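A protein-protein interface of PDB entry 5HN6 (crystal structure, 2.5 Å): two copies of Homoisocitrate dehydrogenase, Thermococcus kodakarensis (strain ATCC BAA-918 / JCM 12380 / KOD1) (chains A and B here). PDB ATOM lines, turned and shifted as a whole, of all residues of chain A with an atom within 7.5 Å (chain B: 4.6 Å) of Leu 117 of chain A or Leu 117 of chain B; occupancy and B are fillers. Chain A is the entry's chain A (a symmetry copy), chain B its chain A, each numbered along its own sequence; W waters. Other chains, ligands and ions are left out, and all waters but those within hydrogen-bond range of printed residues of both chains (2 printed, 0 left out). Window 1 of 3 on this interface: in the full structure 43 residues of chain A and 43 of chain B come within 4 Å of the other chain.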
ATOM      1  N   GLU A 112     -22.171   2.470 -17.281  1.00  0.00           N
ATOM      2  CA  GLU A 112     -22.496   3.873 -17.080  1.00  0.00           C
ATOM      3  C   GLU A 112     -22.905   4.558 -18.429  1.00  0.00           C
ATOM      4  O   GLU A 112     -22.273   4.355 -19.466  1.00  0.00           O
ATOM      5  CB  GLU A 112     -21.359   4.608 -16.372  1.00  0.00           C
ATOM      6  CG  GLU A 112     -21.811   5.901 -15.734  1.00  0.00           C
ATOM      7  CD  GLU A 112     -22.015   7.004 -16.761  1.00  0.00           C
ATOM      8  OE1 GLU A 112     -22.930   7.828 -16.575  1.00  0.00           O
ATOM      9  OE2 GLU A 112     -21.256   7.059 -17.761  1.00  0.00           O
ATOM     10  N   SER A 114     -24.320   8.042 -19.065  1.00  0.00           N
ATOM     11  CA  SER A 114     -24.398   9.509 -19.212  1.00  0.00           C
ATOM     12  C   SER A 114     -23.080  10.240 -19.463  1.00  0.00           C
ATOM     13  O   SER A 114     -23.094  11.337 -20.021  1.00  0.00           O
ATOM     14  CB  SER A 114     -25.005  10.160 -17.971  1.00  0.00           C
ATOM     15  OG  SER A 114     -24.101  10.124 -16.868  1.00  0.00           O
ATOM     16  N   GLU A 115     -21.953   9.686 -19.027  1.00  0.00           N
ATOM     17  CA  GLU A 115     -20.687  10.403 -19.167  1.00  0.00           C
ATOM     18  C   GLU A 115     -19.642   9.531 -19.880  1.00  0.00           C
ATOM     19  O   GLU A 115     -19.974   8.842 -20.853  1.00  0.00           O
ATOM     20  CB  GLU A 115     -20.198  10.998 -17.815  1.00  0.00           C
ATOM     21  CG  GLU A 115     -20.664  10.302 -16.560  1.00  0.00           C
ATOM     22  CD  GLU A 115     -20.091  10.928 -15.299  1.00  0.00           C
ATOM     23  OE1 GLU A 115     -19.382  10.196 -14.574  1.00  0.00           O
ATOM     24  OE2 GLU A 115     -20.360  12.128 -15.020  1.00  0.00           O
ATOM     25  N   GLY A 116     -18.390   9.581 -19.408  1.00  0.00           N
ATOM     26  CA  GLY A 116     -17.291   8.932 -20.042  1.00  0.00           C
ATOM     27  C   GLY A 116     -16.961   9.602 -21.346  1.00  0.00           C
ATOM     28  O   GLY A 116     -17.004  10.832 -21.471  1.00  0.00           O
ATOM     29  N   LEU A 117     -16.605   8.790 -22.325  1.00  0.00           N
ATOM     30  CA  LEU A 117     -16.278   9.321 -23.633  1.00  0.00           C
ATOM     31  C   LEU A 117     -17.539   9.668 -24.429  1.00  0.00           C
ATOM     32  O   LEU A 117     -17.432  10.138 -25.538  1.00  0.00           O
ATOM     33  CB  LEU A 117     -15.399   8.324 -24.390  1.00  0.00           C
ATOM     34  CG  LEU A 117     -13.903   8.522 -24.178  1.00  0.00           C
ATOM     35  CD1 LEU A 117     -13.055   7.351 -24.672  1.00  0.00           C
ATOM     36  CD2 LEU A 117     -13.495   9.833 -24.855  1.00  0.00           C
ATOM     37  N   TYR A 118     -18.715   9.424 -23.856  1.00  0.00           N
ATOM     38  CA  TYR A 118     -20.011   9.842 -24.428  1.00  0.00           C
ATOM     39  C   TYR A 118     -20.448  11.221 -23.899  1.00  0.00           C
ATOM     40  O   TYR A 118     -21.512  11.712 -24.248  1.00  0.00           O
ATOM     41  CB  TYR A 118     -21.124   8.792 -24.078  1.00  0.00           C
ATOM     42  CG  TYR A 118     -21.003   7.502 -24.858  1.00  0.00           C
ATOM     43  CD1 TYR A 118     -19.938   6.630 -24.650  1.00  0.00           C
ATOM     44  CD2 TYR A 118     -21.921   7.167 -25.831  1.00  0.00           C
ATOM     45  CE1 TYR A 118     -19.804   5.455 -25.388  1.00  0.00           C
ATOM     46  CE2 TYR A 118     -21.806   5.977 -26.552  1.00  0.00           C
ATOM     47  CZ  TYR A 118     -20.732   5.145 -26.341  1.00  0.00           C
ATOM     48  OH  TYR A 118     -20.617   3.999 -27.066  1.00  0.00           O
ATOM     49  N   PHE A 119     -19.686  11.861 -23.029  1.00  0.00           N
ATOM     50  CA  PHE A 119     -20.222  13.085 -22.456  1.00  0.00           C
ATOM     51  C   PHE A 119     -20.430  14.198 -23.504  1.00  0.00           C
ATOM     52  O   PHE A 119     -21.241  15.062 -23.302  1.00  0.00           O
ATOM     53  CB  PHE A 119     -19.369  13.593 -21.294  1.00  0.00           C
ATOM     54  CG  PHE A 119     -20.000  14.739 -20.530  1.00  0.00           C
ATOM     55  CD1 PHE A 119     -21.024  14.507 -19.620  1.00  0.00           C
ATOM     56  CD2 PHE A 119     -19.568  16.044 -20.735  1.00  0.00           C
ATOM     57  CE1 PHE A 119     -21.609  15.559 -18.921  1.00  0.00           C
ATOM     58  CE2 PHE A 119     -20.143  17.094 -20.044  1.00  0.00           C
ATOM     59  CZ  PHE A 119     -21.157  16.854 -19.127  1.00  0.00           C
ATOM     60  N   GLY A 120     -19.682  14.190 -24.587  1.00  0.00           N
ATOM     61  CA  GLY A 120     -19.935  15.075 -25.705  1.00  0.00           C
ATOM     62  C   GLY A 120     -18.971  16.233 -25.929  1.00  0.00           C
ATOM     63  O   GLY A 120     -19.218  17.083 -26.771  1.00  0.00           O
ATOM     64  N   ILE A 121     -17.880  16.281 -25.182  1.00  0.00           N
ATOM     65  CA  ILE A 121     -16.888  17.284 -25.387  1.00  0.00           C
ATOM     66  C   ILE A 121     -15.874  16.794 -26.371  1.00  0.00           C
ATOM     67  O   ILE A 121     -15.026  15.994 -26.015  1.00  0.00           O
ATOM     68  CB  ILE A 121     -16.121  17.609 -24.108  1.00  0.00           C
ATOM     69  CG1 ILE A 121     -17.072  18.086 -23.036  1.00  0.00           C
ATOM     70  CG2 ILE A 121     -15.059  18.668 -24.400  1.00  0.00           C
ATOM     71  CD1 ILE A 121     -16.426  18.172 -21.682  1.00  0.00           C
ATOM     72  N   VAL A 130      -9.685  16.017 -30.337  1.00  0.00           N
ATOM     73  CA  VAL A 130      -9.790  15.449 -29.033  1.00  0.00           C
ATOM     74  C   VAL A 130     -11.200  15.026 -28.677  1.00  0.00           C
ATOM     75  O   VAL A 130     -12.177  15.509 -29.218  1.00  0.00           O
ATOM     76  CB  VAL A 130      -9.276  16.422 -27.958  1.00  0.00           C
ATOM     77  CG1 VAL A 130      -7.900  16.923 -28.347  1.00  0.00           C
ATOM     78  CG2 VAL A 130     -10.224  17.592 -27.743  1.00  0.00           C
ATOM     79  N   ASP A 131     -11.291  14.096 -27.738  1.00  0.00           N
ATOM     80  CA  ASP A 131     -12.552  13.761 -27.093  1.00  0.00           C
ATOM     81  C   ASP A 131     -12.182  13.666 -25.643  1.00  0.00           C
ATOM     82  O   ASP A 131     -11.099  13.137 -25.308  1.00  0.00           O
ATOM     83  CB  ASP A 131     -13.057  12.397 -27.582  1.00  0.00           C
ATOM     84  CG  ASP A 131     -13.547  12.426 -28.995  1.00  0.00           C
ATOM     85  OD1 ASP A 131     -14.693  12.861 -29.219  1.00  0.00           O
ATOM     86  OD2 ASP A 131     -12.804  12.021 -29.891  1.00  0.00           O
ATOM     87  N   VAL A 132     -13.075  14.114 -24.783  1.00  0.00           N
ATOM     88  CA  VAL A 132     -12.780  14.224 -23.362  1.00  0.00           C
ATOM     89  C   VAL A 132     -13.575  13.213 -22.593  1.00  0.00           C
ATOM     90  O   VAL A 132     -14.780  13.257 -22.598  1.00  0.00           O
ATOM     91  CB  VAL A 132     -13.053  15.640 -22.800  1.00  0.00           C
ATOM     92  CG1 VAL A 132     -12.705  15.699 -21.326  1.00  0.00           C
ATOM     93  CG2 VAL A 132     -12.226  16.667 -23.562  1.00  0.00           C
ATOM     94  N   ARG A 133     -12.867  12.323 -21.910  1.00  0.00           N
ATOM     95  CA  ARG A 133     -13.464  11.255 -21.125  1.00  0.00           C
ATOM     96  C   ARG A 133     -13.699  11.826 -19.742  1.00  0.00           C
ATOM     97  O   ARG A 133     -12.760  11.993 -18.992  1.00  0.00           O
ATOM     98  CB  ARG A 133     -12.546   9.999 -21.092  1.00  0.00           C
ATOM     99  CG  ARG A 133     -13.252   8.736 -20.637  1.00  0.00           C
ATOM    100  CD  ARG A 133     -12.370   7.453 -20.752  1.00  0.00           C
ATOM    101  NE  ARG A 133     -12.022   7.077 -19.408  1.00  0.00           N
ATOM    102  CZ  ARG A 133     -12.363   5.969 -18.767  1.00  0.00           C
ATOM    103  NH1 ARG A 133     -12.967   4.945 -19.343  1.00  0.00           N
ATOM    104  NH2 ARG A 133     -12.004   5.873 -17.511  1.00  0.00           N
ATOM    105  N   LEU A 134     -14.957  12.108 -19.402  1.00  0.00           N
ATOM    106  CA  LEU A 134     -15.279  12.789 -18.172  1.00  0.00           C
ATOM    107  C   LEU A 134     -15.923  11.852 -17.199  1.00  0.00           C
ATOM    108  O   LEU A 134     -16.915  11.220 -17.521  1.00  0.00           O
ATOM    109  CB  LEU A 134     -16.242  13.945 -18.428  1.00  0.00           C
ATOM    110  CG  LEU A 134     -16.803  14.641 -17.184  1.00  0.00           C
ATOM    111  CD1 LEU A 134     -15.703  15.393 -16.426  1.00  0.00           C
ATOM    112  CD2 LEU A 134     -17.953  15.553 -17.590  1.00  0.00           C
ATOM    113  N   ILE A 135     -15.362  11.785 -16.002  1.00  0.00           N
ATOM    114  CA  ILE A 135     -15.967  11.101 -14.874  1.00  0.00           C
ATOM    115  C   ILE A 135     -16.230  12.173 -13.789  1.00  0.00           C
ATOM    116  O   ILE A 135     -15.318  12.950 -13.459  1.00  0.00           O
ATOM    117  CB  ILE A 135     -15.018  10.004 -14.319  1.00  0.00           C
ATOM    118  CG1 ILE A 135     -14.467   9.102 -15.446  1.00  0.00           C
ATOM    119  CG2 ILE A 135     -15.716   9.170 -13.263  1.00  0.00           C
ATOM    120  CD1 ILE A 135     -15.493   8.237 -16.149  1.00  0.00           C
ATOM    121  N   VAL A 166      -3.567   3.795 -16.474  1.00  0.00           N
ATOM    122  CA  VAL A 166      -3.302   4.784 -17.514  1.00  0.00           C
ATOM    123  C   VAL A 166      -4.218   5.999 -17.396  1.00  0.00           C
ATOM    124  O   VAL A 166      -3.808   7.094 -17.747  1.00  0.00           O
ATOM    125  CB  VAL A 166      -3.494   4.141 -18.905  1.00  0.00           C
ATOM    126  CG1 VAL A 166      -3.406   5.179 -20.025  1.00  0.00           C
ATOM    127  CG2 VAL A 166      -2.469   3.040 -19.147  1.00  0.00           C
ATOM    128  N   LEU A 167      -5.468   5.799 -16.956  1.00  0.00           N
ATOM    129  CA  LEU A 167      -6.505   6.839 -17.038  1.00  0.00           C
ATOM    130  C   LEU A 167      -6.836   7.483 -15.682  1.00  0.00           C
ATOM    131  O   LEU A 167      -7.415   6.831 -14.813  1.00  0.00           O
ATOM    132  CB  LEU A 167      -7.802   6.225 -17.606  1.00  0.00           C
ATOM    133  CG  LEU A 167      -7.710   5.634 -19.006  1.00  0.00           C
ATOM    134  CD1 LEU A 167      -8.974   4.899 -19.406  1.00  0.00           C
ATOM    135  CD2 LEU A 167      -7.388   6.718 -20.006  1.00  0.00           C
ATOM    136  N   THR A 168      -6.490   8.754 -15.499  1.00  0.00           N
ATOM    137  CA  THR A 168      -6.823   9.475 -14.254  1.00  0.00           C
ATOM    138  C   THR A 168      -8.272   9.348 -13.851  1.00  0.00           C
ATOM    139  O   THR A 168      -8.597   9.071 -12.710  1.00  0.00           O
ATOM    140  CB  THR A 168      -6.589  10.927 -14.493  1.00  0.00           C
ATOM    141  OG1 THR A 168      -5.189  11.129 -14.724  1.00  0.00           O
ATOM    142  CG2 THR A 168      -7.111  11.779 -13.346  1.00  0.00           C
ATOM    143  N   GLU A 213     -16.934   2.178 -17.153  1.00  0.00           N
ATOM    144  CA  GLU A 213     -17.230   3.432 -17.861  1.00  0.00           C
ATOM    145  C   GLU A 213     -18.073   3.166 -19.119  1.00  0.00           C
ATOM    146  O   GLU A 213     -18.159   2.040 -19.614  1.00  0.00           O
ATOM    147  CB  GLU A 213     -15.908   4.133 -18.192  1.00  0.00           C
ATOM    148  CG  GLU A 213     -15.969   5.393 -19.029  1.00  0.00           C
ATOM    149  CD  GLU A 213     -16.009   5.083 -20.506  1.00  0.00           C
ATOM    150  OE1 GLU A 213     -16.552   5.907 -21.284  1.00  0.00           O
ATOM    151  OE2 GLU A 213     -15.499   4.008 -20.887  1.00  0.00           O
ATOM    152  N   ASN A 214     -18.702   4.227 -19.606  1.00  0.00           N
ATOM    153  CA  ASN A 214     -19.636   4.169 -20.724  1.00  0.00           C
ATOM    154  C   ASN A 214     -19.157   3.398 -21.942  1.00  0.00           C
ATOM    155  O   ASN A 214     -19.754   2.403 -22.324  1.00  0.00           O
ATOM    156  CB  ASN A 214     -20.052   5.595 -21.127  1.00  0.00           C
ATOM    157  CG  ASN A 214     -21.409   5.644 -21.823  1.00  0.00           C
ATOM    158  OD1 ASN A 214     -21.751   4.791 -22.650  1.00  0.00           O
ATOM    159  ND2 ASN A 214     -22.178   6.653 -21.498  1.00  0.00           N
ATOM    160  N   LEU A 215     -18.076   3.848 -22.549  1.00  0.00           N
ATOM    161  CA  LEU A 215     -17.537   3.180 -23.728  1.00  0.00           C
ATOM    162  C   LEU A 215     -17.003   1.775 -23.445  1.00  0.00           C
ATOM    163  O   LEU A 215     -17.148   0.912 -24.287  1.00  0.00           O
ATOM    164  CB  LEU A 215     -16.466   4.046 -24.386  1.00  0.00           C
ATOM    165  CG  LEU A 215     -15.840   3.470 -25.639  1.00  0.00           C
ATOM    166  CD1 LEU A 215     -16.874   3.299 -26.731  1.00  0.00           C
ATOM    167  CD2 LEU A 215     -14.695   4.330 -26.068  1.00  0.00           C
ATOM    168  N   PHE A 216     -16.404   1.551 -22.277  1.00  0.00           N
ATOM    169  CA  PHE A 216     -15.938   0.204 -21.872  1.00  0.00           C
ATOM    170  C   PHE A 216     -17.106  -0.721 -21.752  1.00  0.00           C
ATOM    171  O   PHE A 216     -17.035  -1.848 -22.143  1.00  0.00           O
ATOM    172  CB  PHE A 216     -15.193   0.246 -20.519  1.00  0.00           C
ATOM    173  CG  PHE A 216     -13.812   0.836 -20.593  1.00  0.00           C
ATOM    174  CD1 PHE A 216     -13.123   0.934 -21.800  1.00  0.00           C
ATOM    175  CD2 PHE A 216     -13.178   1.246 -19.452  1.00  0.00           C
ATOM    176  CE1 PHE A 216     -11.834   1.461 -21.843  1.00  0.00           C
ATOM    177  CE2 PHE A 216     -11.889   1.777 -19.491  1.00  0.00           C
ATOM    178  CZ  PHE A 216     -11.234   1.899 -20.675  1.00  0.00           C
ATOM    179  N   GLU B 115      -0.188   8.305 -28.878  1.00  0.00           N
ATOM    180  CA  GLU B 115      -1.239   9.246 -28.495  1.00  0.00           C
ATOM    181  C   GLU B 115      -2.494   8.499 -28.019  1.00  0.00           C
ATOM    182  O   GLU B 115      -2.380   7.503 -27.292  1.00  0.00           O
ATOM    183  CB  GLU B 115      -1.514  10.300 -29.607  1.00  0.00           C
ATOM    184  CG  GLU B 115      -1.190   9.893 -31.022  1.00  0.00           C
ATOM    185  CD  GLU B 115      -1.543  10.971 -32.034  1.00  0.00           C
ATOM    186  OE1 GLU B 115      -2.385  10.674 -32.910  1.00  0.00           O
ATOM    187  OE2 GLU B 115      -0.973  12.093 -31.974  1.00  0.00           O
ATOM    188  N   GLY B 116      -3.675   8.990 -28.412  1.00  0.00           N
ATOM    189  CA  GLY B 116      -4.923   8.485 -27.946  1.00  0.00           C
ATOM    190  C   GLY B 116      -5.123   8.821 -26.496  1.00  0.00           C
ATOM    191  O   GLY B 116      -4.779   9.914 -26.031  1.00  0.00           O
ATOM    192  N   LEU B 117      -5.706   7.882 -25.773  1.00  0.00           N
ATOM    193  CA  LEU B 117      -5.938   8.087 -24.357  1.00  0.00           C
ATOM    194  C   LEU B 117      -4.660   7.869 -23.542  1.00  0.00           C
ATOM    195  O   LEU B 117      -4.686   8.019 -22.342  1.00  0.00           O
ATOM    196  CB  LEU B 117      -7.065   7.170 -23.879  1.00  0.00           C
ATOM    197  CG  LEU B 117      -8.455   7.786 -23.973  1.00  0.00           C
ATOM    198  CD1 LEU B 117      -9.586   6.774 -23.797  1.00  0.00           C
ATOM    199  CD2 LEU B 117      -8.548   8.912 -22.939  1.00  0.00           C
ATOM    200  N   TYR B 118      -3.562   7.511 -24.203  1.00  0.00           N
ATOM    201  CA  TYR B 118      -2.225   7.414 -23.583  1.00  0.00           C
ATOM    202  C   TYR B 118      -1.438   8.732 -23.718  1.00  0.00           C
ATOM    203  O   TYR B 118      -0.299   8.823 -23.285  1.00  0.00           O
ATOM    204  CB  TYR B 118      -1.397   6.262 -24.256  1.00  0.00           C
ATOM    205  CG  TYR B 118      -1.865   4.877 -23.867  1.00  0.00           C
ATOM    206  CD1 TYR B 118      -3.105   4.394 -24.273  1.00  0.00           C
ATOM    207  CD2 TYR B 118      -1.096   4.064 -23.062  1.00  0.00           C
ATOM    208  CE1 TYR B 118      -3.555   3.131 -23.891  1.00  0.00           C
ATOM    209  CE2 TYR B 118      -1.530   2.787 -22.701  1.00  0.00           C
ATOM    210  CZ  TYR B 118      -2.769   2.344 -23.098  1.00  0.00           C
ATOM    211  OH  TYR B 118      -3.193   1.107 -22.721  1.00  0.00           O
ATOM    212  N   PHE B 119      -1.984   9.759 -24.345  1.00  0.00           N
ATOM    213  CA  PHE B 119      -1.139  10.921 -24.569  1.00  0.00           C
ATOM    214  C   PHE B 119      -0.698  11.605 -23.259  1.00  0.00           C
ATOM    215  O   PHE B 119       0.310  12.260 -23.239  1.00  0.00           O
ATOM    216  CB  PHE B 119      -1.795  11.932 -25.510  1.00  0.00           C
ATOM    217  CG  PHE B 119      -0.871  13.051 -25.942  1.00  0.00           C
ATOM    218  CD1 PHE B 119       0.096  12.837 -26.918  1.00  0.00           C
ATOM    219  CD2 PHE B 119      -0.970  14.311 -25.363  1.00  0.00           C
ATOM    220  CE1 PHE B 119       0.950  13.862 -27.313  1.00  0.00           C
ATOM    221  CE2 PHE B 119      -0.126  15.334 -25.751  1.00  0.00           C
ATOM    222  CZ  PHE B 119       0.828  15.117 -26.734  1.00  0.00           C
ATOM    223  N   ASP B 131      -9.721  12.600 -18.894  1.00  0.00           N
ATOM    224  CA  ASP B 131      -8.561  12.156 -19.653  1.00  0.00           C
ATOM    225  C   ASP B 131      -8.890  12.569 -21.057  1.00  0.00           C
ATOM    226  O   ASP B 131     -10.058  12.444 -21.487  1.00  0.00           O
ATOM    227  CB  ASP B 131      -8.431  10.629 -19.586  1.00  0.00           C
ATOM    228  CG  ASP B 131      -8.001  10.136 -18.241  1.00  0.00           C
ATOM    229  OD1 ASP B 131      -6.791  10.190 -17.946  1.00  0.00           O
ATOM    230  OD2 ASP B 131      -8.854   9.693 -17.469  1.00  0.00           O
ATOM    231  N   VAL B 132      -7.882  13.004 -21.787  1.00  0.00           N
ATOM    232  CA  VAL B 132      -8.089  13.579 -23.109  1.00  0.00           C
ATOM    233  C   VAL B 132      -7.544  12.661 -24.160  1.00  0.00           C
ATOM    234  O   VAL B 132      -6.367  12.399 -24.187  1.00  0.00           O
ATOM    235  CB  VAL B 132      -7.451  14.982 -23.259  1.00  0.00           C
ATOM    236  CG1 VAL B 132      -7.719  15.537 -24.643  1.00  0.00           C
ATOM    237  CG2 VAL B 132      -8.023  15.924 -22.209  1.00  0.00           C
ATOM    238  N   ARG B 133      -8.426  12.204 -25.039  1.00  0.00           N
ATOM    239  CA  ARG B 133      -8.087  11.287 -26.114  1.00  0.00           C
ATOM    240  C   ARG B 133      -7.666  12.147 -27.288  1.00  0.00           C
ATOM    241  O   ARG B 133      -8.506  12.748 -27.926  1.00  0.00           O
ATOM    242  CB  ARG B 133      -9.288  10.362 -26.466  1.00  0.00           C
ATOM    243  CG  ARG B 133      -8.902   9.144 -27.284  1.00  0.00           C
ATOM    244  CD  ARG B 133     -10.080   8.143 -27.502  1.00  0.00           C
ATOM    245  NE  ARG B 133     -10.462   8.260 -28.885  1.00  0.00           N
ATOM    246  CZ  ARG B 133     -10.386   7.328 -29.824  1.00  0.00           C
ATOM    247  NH1 ARG B 133     -10.077   6.067 -29.581  1.00  0.00           N
ATOM    248  NH2 ARG B 133     -10.711   7.683 -31.041  1.00  0.00           N
ATOM    249  N   VAL B 166     -19.356   8.156 -32.314  1.00  0.00           N
ATOM    250  CA  VAL B 166     -19.404   8.845 -31.028  1.00  0.00           C
ATOM    251  C   VAL B 166     -18.210   9.776 -30.833  1.00  0.00           C
ATOM    252  O   VAL B 166     -18.345  10.794 -30.172  1.00  0.00           O
ATOM    253  CB  VAL B 166     -19.428   7.810 -29.882  1.00  0.00           C
ATOM    254  CG1 VAL B 166     -19.296   8.478 -28.513  1.00  0.00           C
ATOM    255  CG2 VAL B 166     -20.705   6.978 -29.923  1.00  0.00           C
ATOM    256  N   LEU B 167     -17.034   9.402 -31.356  1.00  0.00           N
ATOM    257  CA  LEU B 167     -15.774  10.084 -31.022  1.00  0.00           C
ATOM    258  C   LEU B 167     -15.243  10.980 -32.153  1.00  0.00           C
ATOM    259  O   LEU B 167     -14.814  10.476 -33.191  1.00  0.00           O
ATOM    260  CB  LEU B 167     -14.693   9.031 -30.698  1.00  0.00           C
ATOM    261  CG  LEU B 167     -14.980   8.113 -29.519  1.00  0.00           C
ATOM    262  CD1 LEU B 167     -13.956   7.003 -29.389  1.00  0.00           C
ATOM    263  CD2 LEU B 167     -15.058   8.915 -28.243  1.00  0.00           C
ATOM    264  N   GLU B 213      -6.850   3.130 -32.605  1.00  0.00           N
ATOM    265  CA  GLU B 213      -6.276   4.018 -31.584  1.00  0.00           C
ATOM    266  C   GLU B 213      -5.573   3.208 -30.483  1.00  0.00           C
ATOM    267  O   GLU B 213      -5.788   2.003 -30.329  1.00  0.00           O
ATOM    268  CB  GLU B 213      -7.392   4.905 -31.021  1.00  0.00           C
ATOM    269  CG  GLU B 213      -7.049   5.821 -29.866  1.00  0.00           C
ATOM    270  CD  GLU B 213      -7.142   5.108 -28.539  1.00  0.00           C
ATOM    271  OE1 GLU B 213      -6.439   5.517 -27.580  1.00  0.00           O
ATOM    272  OE2 GLU B 213      -7.918   4.132 -28.457  1.00  0.00           O
ATOM    273  N   LEU B 215      -5.525   2.873 -27.002  1.00  0.00           N
ATOM    274  CA  LEU B 215      -6.256   2.056 -26.041  1.00  0.00           C
ATOM    275  C   LEU B 215      -7.114   0.968 -26.688  1.00  0.00           C
ATOM    276  O   LEU B 215      -7.219  -0.105 -26.129  1.00  0.00           O
ATOM    277  CB  LEU B 215      -7.100   2.941 -25.127  1.00  0.00           C
ATOM    278  CG  LEU B 215      -7.895   2.211 -24.065  1.00  0.00           C
ATOM    279  CD1 LEU B 215      -6.977   1.487 -23.103  1.00  0.00           C
ATOM    280  CD2 LEU B 215      -8.804   3.173 -23.370  1.00  0.00           C
HETATM  281  O   HOH W   1     -10.372  11.185 -29.696  1.00  0.00           O
HETATM  282  O   HOH W   2     -11.409   9.581 -17.803  1.00  0.00           O
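Leu 117 of chain A touches its own counterpart, Leu 117 of chain B.
Leu 117 of chain A touches Leu 167 of chain B, and with the chains exchanged Leu 167 of chain A touches Leu 117 of chain B.
Tyr 118 of chain A touches Val 166 of chain B, and with the chains exchanged Val 166 of chain A touches Tyr 118 of chain B.
Asp 131 of chain A touches Val 132 of chain B, and with the chains exchanged Val 132 of chain A touches Asp 131 of chain B.
12 positions are printed for both chains.
Of the 17 pairs that touch across the chains among the printed residues, 13 have their exchanged pair printed and touching as well.
Of the 12 printed residues of chain B, 8 touch a printed residue of chain A.
Printed residues of chain B that touch a printed residue of chain A: Leu 117, Tyr 118, Asp 131, Val 132, Arg 133, Val 166, Leu 167 and Leu 215.
Hydrophobic or aromatic side chains of chain B within 4 Å of the printed part of chain A: Leu 117, Tyr 118, Val 132, Val 166, Leu 167 and Leu 215.
Hydrophobic or aromatic side chains of chain A within 4 Å of the printed part of chain B: Leu 117, Tyr 118, Val 130, Val 166, Leu 167 and Phe 216.
Among the printed residues, no Asp or Glu carboxylate lies within 4 Å of a Lys or Arg side-chain nitrogen of the other chain.
Among the printed residues, merely in contact across the chains: Val 130 of chain A with Arg 133 of chain B, Asp 131 of chain A with Leu 167 of chain B, Leu 167 of chain A with Asp 131 of chain B, Leu 117 of chain A with Leu 117 of chain B, Val 166 of chain A with Tyr 118 of chain B, Tyr 118 of chain A with Val 166 of chain B, Asp 131 of chain A with Val 132 of chain B, Val 132 of chain A with Asp 131 of chain B, Val 130 of chain A with Val 132 of chain B, Phe 216 of chain A with Leu 215 of chain B, Leu 117 of chain A with Leu 167 of chain B, Leu 167 of chain A with Leu 117 of chain B, Val 166 of chain A with Leu 117 of chain B and Leu 117 of chain A with Val 166 of chain B.
Phe 119 of chain A touches none of the printed residues of chain B.
Printed residues of chain B within 4 Å of Phe 216 of chain A: Leu 215 (3.8 Å).
Leu 117 of chain B touches just these residues of chain A: Leu 117, Val 166 and Leu 167.
Of the printed residues of chain A, Tyr 118 of chain B touches Val 166.
Of the printed residues of chain A, Leu 215 of chain B touches Phe 216.
The nearest residue of chain B that does not touch Leu 117 of chain A is Arg 133 of chain B (4.2 Å).
The nearest residue of chain A that does not touch Leu 117 of chain B is Arg 133 of chain A (4.2 Å).
The side-chain carboxylate (OE1) of Glu 213 of chain B is in hydrogen-bond range of the backbone NH (N) of Leu 117 of chain B, at 3.1 Å.
The guanidinium group of Arg 133 of chain B lies within salt-bridge range of the side-chain carboxylate of Glu 213 of chain B, 3.1 Å away.
The side-chain carboxylate (OE1) of Glu 213 of chain A is in hydrogen-bond range of the backbone NH (N) of Leu 117 of chain A.
The backbone carbonyl oxygen (O) of Ile 121 of chain A is in hydrogen-bond range of the backbone NH (N) of Val 132 of chain A.
OE2 of Glu 213 of chain A is in salt-bridge range of NH1 of Arg 133 of chain A (3.1 Å).
N of Phe 216 of chain A is in hydrogen-bond range of OE2 of Glu 213 of chain A (3.0 Å).
O of Asp 131 of chain B is in hydrogen-bond range of N of Arg 133 of chain A.
The side-chain carboxylate of Asp 131 of chain B is in hydrogen-bond range of the backbone NH of Thr 168 of chain A.
The backbone NH of Arg 133 of chain B is in hydrogen-bond range of the backbone carbonyl oxygen of Asp 131 of chain A (2.8 Å).
Water W2 bridges the side-chain carboxylate (OD2) of Asp 131 of chain B (2.6 Å) and the backbone carbonyl oxygen (O) of Arg 133 of chain A (3.0 Å).
Water W1 bridges OD2 of Asp 131 of chain A (2.6 Å) and O of Arg 133 of chain B (3.0 Å).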
